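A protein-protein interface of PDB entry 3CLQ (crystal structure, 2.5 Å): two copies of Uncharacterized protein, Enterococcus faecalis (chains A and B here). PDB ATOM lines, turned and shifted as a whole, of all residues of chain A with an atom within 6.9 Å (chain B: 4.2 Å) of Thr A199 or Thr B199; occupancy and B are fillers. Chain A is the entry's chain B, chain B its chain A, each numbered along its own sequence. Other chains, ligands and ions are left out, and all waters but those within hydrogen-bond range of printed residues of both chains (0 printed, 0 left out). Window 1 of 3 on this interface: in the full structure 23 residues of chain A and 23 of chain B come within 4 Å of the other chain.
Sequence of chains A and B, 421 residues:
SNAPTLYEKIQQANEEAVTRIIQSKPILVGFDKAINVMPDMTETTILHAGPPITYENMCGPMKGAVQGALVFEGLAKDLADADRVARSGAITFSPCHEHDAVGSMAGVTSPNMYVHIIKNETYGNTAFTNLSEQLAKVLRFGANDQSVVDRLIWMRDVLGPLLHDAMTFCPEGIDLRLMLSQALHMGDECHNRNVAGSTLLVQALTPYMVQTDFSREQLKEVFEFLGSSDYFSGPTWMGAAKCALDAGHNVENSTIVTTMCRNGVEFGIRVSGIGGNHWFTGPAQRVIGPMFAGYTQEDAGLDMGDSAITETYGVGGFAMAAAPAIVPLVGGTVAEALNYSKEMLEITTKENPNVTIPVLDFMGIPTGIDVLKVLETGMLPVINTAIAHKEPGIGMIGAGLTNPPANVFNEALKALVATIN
Among the printed residues, pairs that only touch across the chains: Gln A203 with Thr B199 (3.6 Å), Met A186 with Ala B196 (3.6 Å), Gln A203 with Val B202 (3.8 Å) and Met A186 with Val B195 (3.8 Å).
Of the 16 printed residues of chain A, 3 touch a printed residue of chain B. Hydrophobic or aromatic side chains of chain A that line the printed part of chain B: Met A186. Hydrophobic or aromatic side chains of chain B that line the printed part of chain A: Val B195, Ala B196 and Val B202. Among the printed residues, 5 pairs touch across the chains. Among the printed residues, no Asp or Glu carboxylate lies within 4 Å of a Lys or Arg side-chain nitrogen of the other chain.
Thr B199 touches its own counterpart, Thr A199. Gln A203 touches Thr B199, but with the chains exchanged Thr A199 does not touch Gln B203 (4.1 Å). Gln A203 touches Val B202, but with the chains exchanged Val A202 does not touch Gln B203 (4.1 Å). Positions printed for both chains: 195, 196, 197, 198, 199, 200, 201, 202 and 203.
OG1 of Thr A199 is in hydrogen-bond range of O of Val A195, 2.6 Å away.
Thr A199 touches just one residue of chain B: Thr B199. Asp A230 touches none of the printed residues of chain B. Printed residues of chain A within 4 Å of Val B195: Met A186. Of chain A, only Thr A199 and Gln A203 come within 4 Å of Thr B199. Printed residues of chain A within 4 Å of Val B202: Gln A203 (3.8 Å). The nearest residue of chain A that does not touch Thr B199 is Met A186 (4.1 Å).
The side-chain hydroxyl (OG1) of Thr B199 sits close to the backbone carbonyl oxygen (O) of Thr A199, 3.0 Å away.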
ATOM      1  N   MET A 179     -23.843  10.014  26.788  1.00  0.00           N
ATOM      2  CA  MET A 179     -23.603   8.825  25.982  1.00  0.00           C
ATOM      3  C   MET A 179     -22.596   9.131  24.879  1.00  0.00           C
ATOM      4  O   MET A 179     -21.726   8.331  24.554  1.00  0.00           O
ATOM      5  CB  MET A 179     -24.906   8.280  25.412  1.00  0.00           C
ATOM      6  CG  MET A 179     -24.782   6.888  24.846  1.00  0.00           C
ATOM      7  SD  MET A 179     -26.537   6.067  24.449  1.00  0.00           S
ATOM      8  CE  MET A 179     -27.056   5.522  26.267  1.00  0.00           C
ATOM      9  N   MET A 186     -14.717   5.515  23.076  1.00  0.00           N
ATOM     10  CA  MET A 186     -14.782   4.156  22.556  1.00  0.00           C
ATOM     11  C   MET A 186     -14.560   4.086  21.039  1.00  0.00           C
ATOM     12  O   MET A 186     -15.086   3.193  20.360  1.00  0.00           O
ATOM     13  CB  MET A 186     -16.115   3.519  22.886  1.00  0.00           C
ATOM     14  CG  MET A 186     -16.364   3.313  24.350  1.00  0.00           C
ATOM     15  SD  MET A 186     -18.276   3.047  24.714  1.00  0.00           S
ATOM     16  CE  MET A 186     -18.546   1.283  23.951  1.00  0.00           C
ATOM     17  N   ASP A 188     -15.414   6.110  18.529  1.00  0.00           N
ATOM     18  CA  ASP A 188     -16.389   6.657  17.584  1.00  0.00           C
ATOM     19  C   ASP A 188     -16.058   8.091  17.399  1.00  0.00           C
ATOM     20  O   ASP A 188     -15.256   8.628  18.154  1.00  0.00           O
ATOM     21  CB  ASP A 188     -17.787   6.627  18.163  1.00  0.00           C
ATOM     22  CG  ASP A 188     -18.455   5.298  17.975  1.00  0.00           C
ATOM     23  OD1 ASP A 188     -17.705   4.325  17.693  1.00  0.00           O
ATOM     24  OD2 ASP A 188     -19.714   5.240  18.114  1.00  0.00           O
ATOM     25  N   ASN A 194     -20.201   4.840  14.232  1.00  0.00           N
ATOM     26  CA  ASN A 194     -21.244   5.027  15.243  1.00  0.00           C
ATOM     27  C   ASN A 194     -21.496   3.769  16.047  1.00  0.00           C
ATOM     28  O   ASN A 194     -22.495   3.681  16.777  1.00  0.00           O
ATOM     29  CB  ASN A 194     -22.572   5.472  14.584  1.00  0.00           C
ATOM     30  CG  ASN A 194     -22.545   6.922  14.121  1.00  0.00           C
ATOM     31  OD1 ASN A 194     -22.279   7.834  14.919  1.00  0.00           O
ATOM     32  ND2 ASN A 194     -22.821   7.148  12.839  1.00  0.00           N
ATOM     33  N   VAL A 195     -20.571   2.814  15.926  1.00  0.00           N
ATOM     34  CA  VAL A 195     -20.750   1.476  16.489  1.00  0.00           C
ATOM     35  C   VAL A 195     -20.978   1.505  17.991  1.00  0.00           C
ATOM     36  O   VAL A 195     -21.948   0.902  18.505  1.00  0.00           O
ATOM     37  CB  VAL A 195     -19.553   0.523  16.201  1.00  0.00           C
ATOM     38  CG1 VAL A 195     -20.063  -0.935  16.153  1.00  0.00           C
ATOM     39  CG2 VAL A 195     -18.891   0.870  14.900  1.00  0.00           C
ATOM     40  N   ALA A 196     -20.076   2.195  18.689  1.00  0.00           N
ATOM     41  CA  ALA A 196     -20.121   2.255  20.150  1.00  0.00           C
ATOM     42  C   ALA A 196     -21.420   2.904  20.615  1.00  0.00           C
ATOM     43  O   ALA A 196     -22.158   2.336  21.421  1.00  0.00           O
ATOM     44  CB  ALA A 196     -18.950   3.008  20.666  1.00  0.00           C
ATOM     45  N   GLY A 197     -21.708   4.084  20.062  1.00  0.00           N
ATOM     46  CA  GLY A 197     -22.926   4.816  20.376  1.00  0.00           C
ATOM     47  C   GLY A 197     -24.153   3.983  20.113  1.00  0.00           C
ATOM     48  O   GLY A 197     -25.100   3.992  20.896  1.00  0.00           O
ATOM     49  N   SER A 198     -24.142   3.242  19.017  1.00  0.00           N
ATOM     50  CA  SER A 198     -25.338   2.512  18.627  1.00  0.00           C
ATOM     51  C   SER A 198     -25.568   1.379  19.593  1.00  0.00           C
ATOM     52  O   SER A 198     -26.689   1.140  20.041  1.00  0.00           O
ATOM     53  CB  SER A 198     -25.219   2.015  17.191  1.00  0.00           C
ATOM     54  OG  SER A 198     -25.517   3.074  16.284  1.00  0.00           O
ATOM     55  N   THR A 199     -24.483   0.717  19.964  1.00  0.00           N
ATOM     56  CA  THR A 199     -24.545  -0.363  20.929  1.00  0.00           C
ATOM     57  C   THR A 199     -24.874   0.133  22.336  1.00  0.00           C
ATOM     58  O   THR A 199     -25.453  -0.596  23.128  1.00  0.00           O
ATOM     59  CB  THR A 199     -23.212  -1.098  20.915  1.00  0.00           C
ATOM     60  OG1 THR A 199     -22.882  -1.343  19.549  1.00  0.00           O
ATOM     61  CG2 THR A 199     -23.293  -2.416  21.638  1.00  0.00           C
ATOM     62  N   LEU A 200     -24.516   1.365  22.657  1.00  0.00           N
ATOM     63  CA  LEU A 200     -24.859   1.897  23.966  1.00  0.00           C
ATOM     64  C   LEU A 200     -26.329   2.266  24.026  1.00  0.00           C
ATOM     65  O   LEU A 200     -26.943   2.212  25.084  1.00  0.00           O
ATOM     66  CB  LEU A 200     -24.024   3.130  24.321  1.00  0.00           C
ATOM     67  CG  LEU A 200     -22.581   2.892  24.764  1.00  0.00           C
ATOM     68  CD1 LEU A 200     -21.823   4.231  24.686  1.00  0.00           C
ATOM     69  CD2 LEU A 200     -22.438   2.241  26.156  1.00  0.00           C
ATOM     70  N   LEU A 201     -26.886   2.644  22.887  1.00  0.00           N
ATOM     71  CA  LEU A 201     -28.254   3.086  22.825  1.00  0.00           C
ATOM     72  C   LEU A 201     -29.208   1.903  22.829  1.00  0.00           C
ATOM     73  O   LEU A 201     -30.201   1.930  23.553  1.00  0.00           O
ATOM     74  CB  LEU A 201     -28.466   3.900  21.560  1.00  0.00           C
ATOM     75  CG  LEU A 201     -29.328   5.148  21.615  1.00  0.00           C
ATOM     76  CD1 LEU A 201     -30.039   5.386  20.282  1.00  0.00           C
ATOM     77  CD2 LEU A 201     -30.304   5.020  22.703  1.00  0.00           C
ATOM     78  N   VAL A 202     -28.937   0.864  22.041  1.00  0.00           N
ATOM     79  CA  VAL A 202     -29.923  -0.214  21.944  1.00  0.00           C
ATOM     80  C   VAL A 202     -29.979  -0.911  23.290  1.00  0.00           C
ATOM     81  O   VAL A 202     -31.003  -1.445  23.681  1.00  0.00           O
ATOM     82  CB  VAL A 202     -29.659  -1.258  20.797  1.00  0.00           C
ATOM     83  CG1 VAL A 202     -28.905  -0.659  19.613  1.00  0.00           C
ATOM     84  CG2 VAL A 202     -28.945  -2.507  21.314  1.00  0.00           C
ATOM     85  N   GLN A 203     -28.863  -0.883  24.005  1.00  0.00           N
ATOM     86  CA  GLN A 203     -28.796  -1.462  25.318  1.00  0.00           C
ATOM     87  C   GLN A 203     -29.588  -0.656  26.377  1.00  0.00           C
ATOM     88  O   GLN A 203     -30.248  -1.223  27.242  1.00  0.00           O
ATOM     89  CB  GLN A 203     -27.338  -1.589  25.750  1.00  0.00           C
ATOM     90  CG  GLN A 203     -27.204  -2.294  27.061  1.00  0.00           C
ATOM     91  CD  GLN A 203     -25.849  -2.121  27.681  1.00  0.00           C
ATOM     92  OE1 GLN A 203     -25.087  -1.196  27.331  1.00  0.00           O
ATOM     93  NE2 GLN A 203     -25.521  -3.008  28.614  1.00  0.00           N
ATOM     94  N   ALA A 204     -29.506   0.660  26.327  1.00  0.00           N
ATOM     95  CA  ALA A 204     -30.264   1.468  27.256  1.00  0.00           C
ATOM     96  C   ALA A 204     -31.766   1.355  26.958  1.00  0.00           C
ATOM     97  O   ALA A 204     -32.594   1.404  27.866  1.00  0.00           O
ATOM     98  CB  ALA A 204     -29.805   2.909  27.199  1.00  0.00           C
ATOM     99  N   ASP A 230     -24.796  -0.789  11.949  1.00  0.00           N
ATOM    100  CA  ASP A 230     -24.286  -0.078  13.105  1.00  0.00           C
ATOM    101  C   ASP A 230     -24.660   1.405  13.083  1.00  0.00           C
ATOM    102  O   ASP A 230     -24.119   2.178  13.839  1.00  0.00           O
ATOM    103  CB  ASP A 230     -22.783  -0.307  13.287  1.00  0.00           C
ATOM    104  CG  ASP A 230     -21.963   0.317  12.189  1.00  0.00           C
ATOM    105  OD1 ASP A 230     -20.694   0.237  12.254  1.00  0.00           O
ATOM    106  OD2 ASP A 230     -22.586   0.894  11.269  1.00  0.00           O
ATOM    107  N   SER A 233     -27.704   4.887  15.888  1.00  0.00           N
ATOM    108  CA  SER A 233     -27.584   6.092  16.712  1.00  0.00           C
ATOM    109  C   SER A 233     -27.083   7.336  15.951  1.00  0.00           C
ATOM    110  O   SER A 233     -26.974   8.433  16.530  1.00  0.00           O
ATOM    111  CB  SER A 233     -26.634   5.816  17.876  1.00  0.00           C
ATOM    112  OG  SER A 233     -25.319   5.661  17.389  1.00  0.00           O
ATOM    113  N   VAL B 195     -15.819  -1.908  28.604  1.00  0.00           N
ATOM    114  CA  VAL B 195     -17.039  -1.214  28.226  1.00  0.00           C
ATOM    115  C   VAL B 195     -17.578  -1.752  26.907  1.00  0.00           C
ATOM    116  O   VAL B 195     -18.712  -2.194  26.819  1.00  0.00           O
ATOM    117  CB  VAL B 195     -16.830   0.296  28.063  1.00  0.00           C
ATOM    118  CG1 VAL B 195     -18.164   0.964  27.894  1.00  0.00           C
ATOM    119  CG2 VAL B 195     -16.141   0.852  29.257  1.00  0.00           C
ATOM    120  N   ALA B 196     -16.762  -1.711  25.870  1.00  0.00           N
ATOM    121  CA  ALA B 196     -17.265  -2.050  24.556  1.00  0.00           C
ATOM    122  C   ALA B 196     -17.630  -3.530  24.500  1.00  0.00           C
ATOM    123  O   ALA B 196     -18.654  -3.902  23.893  1.00  0.00           O
ATOM    124  CB  ALA B 196     -16.264  -1.691  23.481  1.00  0.00           C
ATOM    125  N   GLY B 197     -16.802  -4.350  25.149  1.00  0.00           N
ATOM    126  CA  GLY B 197     -16.956  -5.782  25.136  1.00  0.00           C
ATOM    127  C   GLY B 197     -18.218  -6.192  25.838  1.00  0.00           C
ATOM    128  O   GLY B 197     -18.918  -7.081  25.397  1.00  0.00           O
ATOM    129  N   SER B 198     -18.540  -5.543  26.939  1.00  0.00           N
ATOM    130  CA  SER B 198     -19.727  -5.924  27.643  1.00  0.00           C
ATOM    131  C   SER B 198     -20.941  -5.505  26.835  1.00  0.00           C
ATOM    132  O   SER B 198     -21.966  -6.223  26.751  1.00  0.00           O
ATOM    133  CB  SER B 198     -19.717  -5.241  28.973  1.00  0.00           C
ATOM    134  OG  SER B 198     -18.658  -5.783  29.701  1.00  0.00           O
ATOM    135  N   THR B 199     -20.836  -4.367  26.183  1.00  0.00           N
ATOM    136  CA  THR B 199     -21.996  -3.967  25.410  1.00  0.00           C
ATOM    137  C   THR B 199     -22.245  -4.832  24.160  1.00  0.00           C
ATOM    138  O   THR B 199     -23.388  -5.118  23.809  1.00  0.00           O
ATOM    139  CB  THR B 199     -22.056  -2.483  25.137  1.00  0.00           C
ATOM    140  OG1 THR B 199     -23.268  -2.251  24.460  1.00  0.00           O
ATOM    141  CG2 THR B 199     -20.941  -2.029  24.252  1.00  0.00           C
ATOM    142  N   LEU B 200     -21.179  -5.297  23.524  1.00  0.00           N
ATOM    143  CA  LEU B 200     -21.342  -6.268  22.458  1.00  0.00           C
ATOM    144  C   LEU B 200     -21.957  -7.560  23.016  1.00  0.00           C
ATOM    145  O   LEU B 200     -22.936  -8.065  22.469  1.00  0.00           O
ATOM    146  CB  LEU B 200     -20.026  -6.539  21.720  1.00  0.00           C
ATOM    147  CG  LEU B 200     -19.391  -5.314  21.039  1.00  0.00           C
ATOM    148  CD1 LEU B 200     -17.926  -5.525  20.828  1.00  0.00           C
ATOM    149  CD2 LEU B 200     -20.043  -4.977  19.710  1.00  0.00           C
ATOM    150  N   LEU B 201     -21.428  -8.067  24.116  1.00  0.00           N
ATOM    151  CA  LEU B 201     -21.975  -9.282  24.679  1.00  0.00           C
ATOM    152  C   LEU B 201     -23.482  -9.196  24.910  1.00  0.00           C
ATOM    153  O   LEU B 201     -24.221 -10.033  24.387  1.00  0.00           O
ATOM    154  CB  LEU B 201     -21.304  -9.624  25.980  1.00  0.00           C
ATOM    155  CG  LEU B 201     -20.699 -11.024  26.077  1.00  0.00           C
ATOM    156  CD1 LEU B 201     -20.620 -11.414  27.548  1.00  0.00           C
ATOM    157  CD2 LEU B 201     -21.450 -12.066  25.257  1.00  0.00           C
ATOM    158  N   VAL B 202     -23.963  -8.193  25.656  1.00  0.00           N
ATOM    159  CA  VAL B 202     -25.392  -8.196  25.948  1.00  0.00           C
ATOM    160  C   VAL B 202     -26.223  -7.980  24.690  1.00  0.00           C
ATOM    161  O   VAL B 202     -27.352  -8.501  24.585  1.00  0.00           O
ATOM    162  CB  VAL B 202     -25.852  -7.254  27.108  1.00  0.00           C
ATOM    163  CG1 VAL B 202     -24.720  -6.910  28.039  1.00  0.00           C
ATOM    164  CG2 VAL B 202     -26.579  -6.014  26.589  1.00  0.00           C
ATOM    165  N   GLN B 203     -25.687  -7.233  23.731  1.00  0.00           N
ATOM    166  CA  GLN B 203     -26.431  -7.108  22.487  1.00  0.00           C
ATOM    167  C   GLN B 203     -26.593  -8.514  21.912  1.00  0.00           C
ATOM    168  O   GLN B 203     -27.711  -8.953  21.566  1.00  0.00           O
ATOM    169  CB  GLN B 203     -25.726  -6.207  21.467  1.00  0.00           C
ATOM    170  CG  GLN B 203     -26.600  -5.842  20.282  1.00  0.00           C
ATOM    171  CD  GLN B 203     -25.849  -5.095  19.170  1.00  0.00           C
ATOM    172  OE1 GLN B 203     -24.626  -5.253  18.998  1.00  0.00           O
ATOM    173  NE2 GLN B 203     -26.582  -4.285  18.405  1.00  0.00           N
